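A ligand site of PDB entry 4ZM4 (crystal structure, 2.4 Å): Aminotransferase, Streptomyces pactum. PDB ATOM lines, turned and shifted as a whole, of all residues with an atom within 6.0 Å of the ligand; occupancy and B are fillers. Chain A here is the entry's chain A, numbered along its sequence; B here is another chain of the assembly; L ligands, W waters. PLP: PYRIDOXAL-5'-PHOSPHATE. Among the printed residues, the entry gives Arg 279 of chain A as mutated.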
ATOM      1  N   ASN A 121      -2.116 -18.298  16.139  1.00  0.00           N
ATOM      2  CA  ASN A 121      -2.557 -17.208  16.983  1.00  0.00           C
ATOM      3  C   ASN A 121      -2.534 -15.826  16.324  1.00  0.00           C
ATOM      4  O   ASN A 121      -3.166 -14.909  16.822  1.00  0.00           O
ATOM      5  CB  ASN A 121      -1.721 -17.191  18.263  1.00  0.00           C
ATOM      6  CG  ASN A 121      -1.747 -18.516  18.980  1.00  0.00           C
ATOM      7  OD1 ASN A 121      -2.794 -18.927  19.490  1.00  0.00           O
ATOM      8  ND2 ASN A 121      -0.594 -19.201  19.024  1.00  0.00           N
ATOM      9  N   SER A 122      -1.775 -15.671  15.260  1.00  0.00           N
ATOM     10  CA  SER A 122      -1.487 -14.345  14.689  1.00  0.00           C
ATOM     11  C   SER A 122      -1.126 -14.434  13.244  1.00  0.00           C
ATOM     12  O   SER A 122      -0.713 -15.501  12.758  1.00  0.00           O
ATOM     13  CB  SER A 122      -0.319 -13.747  15.429  1.00  0.00           C
ATOM     14  OG  SER A 122       0.847 -14.508  15.205  1.00  0.00           O
ATOM     15  N   GLY A 123      -1.304 -13.341  12.517  1.00  0.00           N
ATOM     16  CA  GLY A 123      -0.882 -13.288  11.108  1.00  0.00           C
ATOM     17  C   GLY A 123       0.629 -13.557  10.941  1.00  0.00           C
ATOM     18  O   GLY A 123       1.054 -14.175   9.972  1.00  0.00           O
ATOM     19  N   THR A 124       1.418 -13.079  11.904  1.00  0.00           N
ATOM     20  CA  THR A 124       2.846 -13.280  11.903  1.00  0.00           C
ATOM     21  C   THR A 124       3.196 -14.785  11.927  1.00  0.00           C
ATOM     22  O   THR A 124       3.973 -15.267  11.063  1.00  0.00           O
ATOM     23  CB  THR A 124       3.507 -12.538  13.055  1.00  0.00           C
ATOM     24  OG1 THR A 124       3.442 -11.120  12.825  1.00  0.00           O
ATOM     25  CG2 THR A 124       4.965 -12.971  13.249  1.00  0.00           C
ATOM     26  N   GLU A 125       2.577 -15.511  12.832  1.00  0.00           N
ATOM     27  CA  GLU A 125       2.724 -16.980  12.886  1.00  0.00           C
ATOM     28  C   GLU A 125       2.230 -17.686  11.614  1.00  0.00           C
ATOM     29  O   GLU A 125       2.920 -18.570  11.087  1.00  0.00           O
ATOM     30  CB  GLU A 125       1.991 -17.589  14.124  1.00  0.00           C
ATOM     31  CG  GLU A 125       2.637 -17.302  15.472  1.00  0.00           C
ATOM     32  CD  GLU A 125       1.897 -17.976  16.621  1.00  0.00           C
ATOM     33  OE1 GLU A 125       0.743 -18.405  16.442  1.00  0.00           O
ATOM     34  OE2 GLU A 125       2.497 -18.065  17.712  1.00  0.00           O
ATOM     35  N   VAL A 127       1.840 -16.532   8.549  1.00  0.00           N
ATOM     36  CA  VAL A 127       2.758 -16.218   7.477  1.00  0.00           C
ATOM     37  C   VAL A 127       4.035 -17.084   7.572  1.00  0.00           C
ATOM     38  O   VAL A 127       4.448 -17.679   6.566  1.00  0.00           O
ATOM     39  CB  VAL A 127       3.058 -14.688   7.448  1.00  0.00           C
ATOM     40  CG1 VAL A 127       4.307 -14.350   6.628  1.00  0.00           C
ATOM     41  CG2 VAL A 127       1.861 -13.895   6.900  1.00  0.00           C
ATOM     42  N   TYR A 150       3.306  -5.631   4.188  1.00  0.00           N
ATOM     43  CA  TYR A 150       3.687  -6.108   5.500  1.00  0.00           C
ATOM     44  C   TYR A 150       3.108  -7.495   5.750  1.00  0.00           C
ATOM     45  O   TYR A 150       1.921  -7.748   5.559  1.00  0.00           O
ATOM     46  CB  TYR A 150       3.234  -5.085   6.567  1.00  0.00           C
ATOM     47  CG  TYR A 150       3.578  -5.466   8.007  1.00  0.00           C
ATOM     48  CD1 TYR A 150       4.910  -5.515   8.437  1.00  0.00           C
ATOM     49  CD2 TYR A 150       2.590  -5.792   8.910  1.00  0.00           C
ATOM     50  CE1 TYR A 150       5.230  -5.848   9.744  1.00  0.00           C
ATOM     51  CE2 TYR A 150       2.901  -6.149  10.219  1.00  0.00           C
ATOM     52  CZ  TYR A 150       4.223  -6.200  10.626  1.00  0.00           C
ATOM     53  OH  TYR A 150       4.506  -6.579  11.900  1.00  0.00           O
ATOM     54  N   HIS A 151       3.982  -8.413   6.187  1.00  0.00           N
ATOM     55  CA  HIS A 151       3.564  -9.802   6.432  1.00  0.00           C
ATOM     56  C   HIS A 151       3.857 -10.297   7.844  1.00  0.00           C
ATOM     57  O   HIS A 151       4.076 -11.482   8.094  1.00  0.00           O
ATOM     58  CB  HIS A 151       4.197 -10.683   5.345  1.00  0.00           C
ATOM     59  CG  HIS A 151       3.867 -10.220   3.962  1.00  0.00           C
ATOM     60  ND1 HIS A 151       2.577 -10.060   3.538  1.00  0.00           N
ATOM     61  CD2 HIS A 151       4.657  -9.795   2.937  1.00  0.00           C
ATOM     62  CE1 HIS A 151       2.569  -9.591   2.300  1.00  0.00           C
ATOM     63  NE2 HIS A 151       3.827  -9.431   1.909  1.00  0.00           N
ATOM     64  N   GLY A 152       3.851  -9.371   8.786  1.00  0.00           N
ATOM     65  CA  GLY A 152       4.201  -9.697  10.182  1.00  0.00           C
ATOM     66  C   GLY A 152       5.698  -9.571  10.410  1.00  0.00           C
ATOM     67  O   GLY A 152       6.439  -9.141   9.520  1.00  0.00           O
ATOM     68  N   TRP A 153       6.153  -9.990  11.574  1.00  0.00           N
ATOM     69  CA  TRP A 153       7.490  -9.691  12.020  1.00  0.00           C
ATOM     70  C   TRP A 153       8.393 -10.915  12.151  1.00  0.00           C
ATOM     71  O   TRP A 153       9.436 -10.822  12.801  1.00  0.00           O
ATOM     72  CB  TRP A 153       7.450  -8.925  13.367  1.00  0.00           C
ATOM     73  CG  TRP A 153       6.562  -9.514  14.403  1.00  0.00           C
ATOM     74  CD1 TRP A 153       5.197  -9.337  14.512  1.00  0.00           C
ATOM     75  CD2 TRP A 153       6.963 -10.312  15.522  1.00  0.00           C
ATOM     76  NE1 TRP A 153       4.718 -10.025  15.620  1.00  0.00           N
ATOM     77  CE2 TRP A 153       5.791 -10.618  16.267  1.00  0.00           C
ATOM     78  CE3 TRP A 153       8.184 -10.758  15.983  1.00  0.00           C
ATOM     79  CZ2 TRP A 153       5.821 -11.401  17.423  1.00  0.00           C
ATOM     80  CZ3 TRP A 153       8.210 -11.493  17.122  1.00  0.00           C
ATOM     81  CH2 TRP A 153       7.029 -11.819  17.833  1.00  0.00           C
ATOM     82  N   GLU A 218       0.149  -8.599  -0.490  1.00  0.00           N
ATOM     83  CA  GLU A 218      -1.139  -8.045  -0.066  1.00  0.00           C
ATOM     84  C   GLU A 218      -1.927  -7.752  -1.341  1.00  0.00           C
ATOM     85  O   GLU A 218      -1.582  -6.818  -2.052  1.00  0.00           O
ATOM     86  CB  GLU A 218      -0.973  -6.751   0.746  1.00  0.00           C
ATOM     87  CG  GLU A 218      -0.433  -6.927   2.153  1.00  0.00           C
ATOM     88  CD  GLU A 218      -0.429  -5.612   2.924  1.00  0.00           C
ATOM     89  OE1 GLU A 218      -1.443  -4.903   2.941  1.00  0.00           O
ATOM     90  OE2 GLU A 218       0.644  -5.248   3.498  1.00  0.00           O
ATOM     91  N   ASN A 223      -1.389  -1.704   4.279  1.00  0.00           N
ATOM     92  CA  ASN A 223      -0.439  -1.101   5.254  1.00  0.00           C
ATOM     93  C   ASN A 223       0.475   0.035   4.710  1.00  0.00           C
ATOM     94  O   ASN A 223       1.511   0.362   5.304  1.00  0.00           O
ATOM     95  CB  ASN A 223       0.469  -2.195   5.843  1.00  0.00           C
ATOM     96  CG  ASN A 223      -0.289  -3.224   6.666  1.00  0.00           C
ATOM     97  OD1 ASN A 223      -0.561  -3.029   7.865  1.00  0.00           O
ATOM     98  ND2 ASN A 223      -0.534  -4.369   6.077  1.00  0.00           N
ATOM     99  N   ASP A 251      -1.616 -12.750   1.192  1.00  0.00           N
ATOM    100  CA  ASP A 251      -1.799 -12.356   2.579  1.00  0.00           C
ATOM    101  C   ASP A 251      -3.086 -11.605   2.644  1.00  0.00           C
ATOM    102  O   ASP A 251      -3.127 -10.401   2.343  1.00  0.00           O
ATOM    103  CB  ASP A 251      -0.623 -11.486   3.068  1.00  0.00           C
ATOM    104  CG  ASP A 251      -0.689 -11.185   4.536  1.00  0.00           C
ATOM    105  OD1 ASP A 251      -1.738 -11.414   5.159  1.00  0.00           O
ATOM    106  OD2 ASP A 251       0.313 -10.675   5.091  1.00  0.00           O
ATOM    107  N   GLU A 252      -4.144 -12.303   3.043  1.00  0.00           N
ATOM    108  CA  GLU A 252      -5.453 -11.656   3.191  1.00  0.00           C
ATOM    109  C   GLU A 252      -5.825 -11.400   4.665  1.00  0.00           C
ATOM    110  O   GLU A 252      -6.997 -11.363   5.024  1.00  0.00           O
ATOM    111  CB  GLU A 252      -6.523 -12.491   2.511  1.00  0.00           C
ATOM    112  CG  GLU A 252      -6.302 -12.599   0.993  1.00  0.00           C
ATOM    113  CD  GLU A 252      -7.572 -12.355   0.195  1.00  0.00           C
ATOM    114  OE1 GLU A 252      -8.289 -11.396   0.539  1.00  0.00           O
ATOM    115  OE2 GLU A 252      -7.840 -13.096  -0.770  1.00  0.00           O
ATOM    116  N   VAL A 253      -4.809 -11.189   5.500  1.00  0.00           N
ATOM    117  CA  VAL A 253      -5.003 -10.919   6.913  1.00  0.00           C
ATOM    118  C   VAL A 253      -5.928  -9.756   7.037  1.00  0.00           C
ATOM    119  O   VAL A 253      -6.850  -9.768   7.873  1.00  0.00           O
ATOM    120  CB  VAL A 253      -3.641 -10.635   7.647  1.00  0.00           C
ATOM    121  CG1 VAL A 253      -3.856  -9.824   8.916  1.00  0.00           C
ATOM    122  CG2 VAL A 253      -2.980 -11.963   7.970  1.00  0.00           C
ATOM    123  N   ILE A 254      -5.740  -8.742   6.205  1.00  0.00           N
ATOM    124  CA  ILE A 254      -6.618  -7.551   6.233  1.00  0.00           C
ATOM    125  C   ILE A 254      -7.783  -7.686   5.233  1.00  0.00           C
ATOM    126  O   ILE A 254      -8.938  -7.467   5.602  1.00  0.00           O
ATOM    127  CB  ILE A 254      -5.832  -6.260   5.988  1.00  0.00           C
ATOM    128  CG1 ILE A 254      -5.114  -5.872   7.244  1.00  0.00           C
ATOM    129  CG2 ILE A 254      -6.753  -5.111   5.576  1.00  0.00           C
ATOM    130  CD1 ILE A 254      -4.138  -4.707   7.056  1.00  0.00           C
ATOM    131  N   SER A 278      -6.896 -13.786   9.056  1.00  0.00           N
ATOM    132  CA  SER A 278      -6.957 -13.408  10.456  1.00  0.00           C
ATOM    133  C   SER A 278      -8.009 -12.303  10.599  1.00  0.00           C
ATOM    134  O   SER A 278      -8.889 -12.188   9.785  1.00  0.00           O
ATOM    135  CB  SER A 278      -5.584 -12.916  10.929  1.00  0.00           C
ATOM    136  OG  SER A 278      -5.564 -12.698  12.344  1.00  0.00           O
ATOM    137  N   ARG A 279      -7.925 -11.494  11.646  1.00  0.00           N
ATOM    138  CA  ARG A 279      -8.699 -10.213  11.752  1.00  0.00           C
ATOM    139  C   ARG A 279     -10.201 -10.377  11.755  1.00  0.00           C
ATOM    140  O   ARG A 279     -10.758 -10.685  12.788  1.00  0.00           O
ATOM    141  CB  ARG A 279      -8.272  -9.205  10.700  1.00  0.00           C
ATOM    142  CG  ARG A 279      -6.810  -8.905  10.697  1.00  0.00           C
ATOM    143  CD  ARG A 279      -6.364  -7.976  11.801  1.00  0.00           C
ATOM    144  NE  ARG A 279      -4.941  -8.208  12.005  1.00  0.00           N
ATOM    145  CZ  ARG A 279      -3.938  -7.445  11.565  1.00  0.00           C
ATOM    146  NH1 ARG A 279      -4.130  -6.280  10.923  1.00  0.00           N
ATOM    147  NH2 ARG A 279      -2.712  -7.858  11.845  1.00  0.00           N
ATOM    148  N   ASN B 121       1.185 -13.023  21.812  1.00  0.00           N
ATOM    149  CA  ASN B 121       0.102 -13.996  21.746  1.00  0.00           C
ATOM    150  C   ASN B 121       0.540 -15.403  22.143  1.00  0.00           C
ATOM    151  O   ASN B 121      -0.299 -16.240  22.434  1.00  0.00           O
ATOM    152  CB  ASN B 121      -0.472 -14.040  20.327  1.00  0.00           C
ATOM    153  CG  ASN B 121      -0.906 -12.691  19.871  1.00  0.00           C
ATOM    154  OD1 ASN B 121      -1.864 -12.117  20.421  1.00  0.00           O
ATOM    155  ND2 ASN B 121      -0.216 -12.137  18.861  1.00  0.00           N
ATOM    156  N   GLU B 125       6.272 -16.386  20.057  1.00  0.00           N
ATOM    157  CA  GLU B 125       6.445 -14.941  19.761  1.00  0.00           C
ATOM    158  C   GLU B 125       7.269 -14.246  20.851  1.00  0.00           C
ATOM    159  O   GLU B 125       8.162 -13.463  20.559  1.00  0.00           O
ATOM    160  CB  GLU B 125       5.088 -14.228  19.614  1.00  0.00           C
ATOM    161  CG  GLU B 125       4.331 -14.496  18.332  1.00  0.00           C
ATOM    162  CD  GLU B 125       3.011 -13.736  18.240  1.00  0.00           C
ATOM    163  OE1 GLU B 125       2.541 -13.166  19.271  1.00  0.00           O
ATOM    164  OE2 GLU B 125       2.445 -13.708  17.139  1.00  0.00           O
ATOM    165  N   ALA B 308       6.128  -6.669  18.149  1.00  0.00           N
ATOM    166  CA  ALA B 308       4.907  -6.272  17.426  1.00  0.00           C
ATOM    167  C   ALA B 308       3.811  -7.310  17.549  1.00  0.00           C
ATOM    168  O   ALA B 308       3.972  -8.307  18.265  1.00  0.00           O
ATOM    169  CB  ALA B 308       5.252  -6.009  15.949  1.00  0.00           C
ATOM    170  N   GLY B 309       2.724  -7.090  16.806  1.00  0.00           N
ATOM    171  CA  GLY B 309       1.607  -8.016  16.746  1.00  0.00           C
ATOM    172  C   GLY B 309       0.344  -7.270  17.116  1.00  0.00           C
ATOM    173  O   GLY B 309       0.210  -6.778  18.226  1.00  0.00           O
ATOM    174  N   VAL B 310      -0.556  -7.185  16.156  1.00  0.00           N
ATOM    175  CA  VAL B 310      -1.736  -6.371  16.315  1.00  0.00           C
ATOM    176  C   VAL B 310      -2.535  -6.776  17.571  1.00  0.00           C
ATOM    177  O   VAL B 310      -3.141  -5.924  18.212  1.00  0.00           O
ATOM    178  CB  VAL B 310      -2.619  -6.432  15.025  1.00  0.00           C
ATOM    179  CG1 VAL B 310      -3.533  -7.649  15.037  1.00  0.00           C
ATOM    180  CG2 VAL B 310      -3.462  -5.192  14.875  1.00  0.00           C
ATOM    181  N   TYR B 311      -2.537  -8.076  17.893  1.00  0.00           N
ATOM    182  CA  TYR B 311      -3.297  -8.607  19.050  1.00  0.00           C
ATOM    183  C   TYR B 311      -2.523  -8.565  20.360  1.00  0.00           C
ATOM    184  O   TYR B 311      -3.032  -8.986  21.413  1.00  0.00           O
ATOM    185  CB  TYR B 311      -3.685 -10.080  18.811  1.00  0.00           C
ATOM    186  CG  TYR B 311      -4.550 -10.364  17.617  1.00  0.00           C
ATOM    187  CD1 TYR B 311      -5.834  -9.818  17.512  1.00  0.00           C
ATOM    188  CD2 TYR B 311      -4.110 -11.190  16.608  1.00  0.00           C
ATOM    189  CE1 TYR B 311      -6.632 -10.054  16.408  1.00  0.00           C
ATOM    190  CE2 TYR B 311      -4.906 -11.457  15.510  1.00  0.00           C
ATOM    191  CZ  TYR B 311      -6.170 -10.900  15.422  1.00  0.00           C
ATOM    192  OH  TYR B 311      -6.956 -11.166  14.325  1.00  0.00           O
HETATM  193  N1  PLP L   1      -0.335  -9.391   7.438  1.00  0.00           N
HETATM  194  C2  PLP L   1      -0.846  -8.176   7.220  1.00  0.00           C
HETATM  195  C2A PLP L   1      -1.323  -7.899   5.837  1.00  0.00           C
HETATM  196  C3  PLP L   1      -0.968  -7.164   8.304  1.00  0.00           C
HETATM  197  O3  PLP L   1      -1.501  -5.934   8.054  1.00  0.00           O
HETATM  198  C4  PLP L   1      -0.484  -7.539   9.676  1.00  0.00           C
HETATM  199  C4A PLP L   1      -0.476  -6.500  10.748  1.00  0.00           C
HETATM  200  O4A PLP L   1      -0.579  -5.270  10.442  1.00  0.00           O
HETATM  201  C5  PLP L   1       0.060  -8.931   9.767  1.00  0.00           C
HETATM  202  C6  PLP L   1       0.117  -9.754   8.639  1.00  0.00           C
HETATM  203  C5A PLP L   1       0.600  -9.544  11.024  1.00  0.00           C
HETATM  204  O4P PLP L   1      -0.439 -10.164  11.830  1.00  0.00           O
HETATM  205  P   PLP L   1      -0.244  -9.970  13.438  1.00  0.00           P
HETATM  206  O1P PLP L   1       1.104 -10.686  13.680  1.00  0.00           O
HETATM  207  O2P PLP L   1      -1.442 -10.639  14.083  1.00  0.00           O
HETATM  208  O3P PLP L   1      -0.077  -8.497  13.705  1.00  0.00           O
HETATM  209  O   HOH W   1      -0.871 -10.214  16.704  1.00  0.00           O
HETATM  210  O   HOH W   2       1.766 -10.987  16.161  1.00  0.00           O
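The backbone carbonyl oxygen of Tyr 311 of chain B sits close to the side-chain amide oxygen of Asn 121 of chain B (3.5 Å). OE2 of Glu 218 sits at hydrogen-bond distance from N of Tyr 150 (2.8 Å). OH of Tyr 311 of chain B lies within hydrogen-bond range of N of Arg 279 (2.9 Å). The side-chain hydroxyl of Thr 124 sits close to the backbone NH of Trp 153 (3.2 Å). N of Val 253 lies within hydrogen-bond range of OD1 of Asp 251 (3.1 Å). The side-chain hydroxyl of Ser 122 is in hydrogen-bond range of the backbone NH of Glu 125 of chain A. The side-chain hydroxyl of Ser 122 is in hydrogen-bond range of the side-chain carboxylate of Glu 125 of chain B, at 2.6 Å. ND2 of Asn 223 sits at hydrogen-bond distance from OE2 of Glu 218, at 3.0 Å.
Water W2 lies within hydrogen-bond range of O1P of the ligand, OE2 of Glu 125 of chain B and NE1 of Trp 153.
A nitrogen (N1) of the ligand lies close to the backbone carbonyl oxygen (O) of Tyr 150 (3.4 Å). Merely in contact with the ligand: Ile 254, Gly 309 of chain B, Val 253, Ser 122, Gly 152, Tyr 311 of chain B, Glu 218 and His 151. Hydrophobic or aromatic side chains within 4 Å of the ligand: Tyr 150, Val 253, Ile 254, Val 310 of chain B and Tyr 311 of chain B.
O3P of the ligand lies within salt-bridge range of NH2 of Arg 279 (3.3 Å). The backbone NH (N) of Thr 124 sits at hydrogen-bond distance from an oxygen (O1P) of the ligand (3.0 Å). The backbone NH (N) of Val 310 of chain B lies within hydrogen-bond range of an oxygen (O3P) of the ligand. ND2 of Asn 223 lies within hydrogen-bond range of O3 of the ligand (2.7 Å). An oxygen (O2P) of the ligand lies within hydrogen-bond range of the backbone NH (N) of Gly 123, 3.1 Å away. The side-chain hydroxyl (OG1) of Thr 124 lies within hydrogen-bond range of an oxygen (O1P) of the ligand (2.5 Å). OD2 of Asp 251 sits at hydrogen-bond distance from N1 of the ligand, at 2.8 Å.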
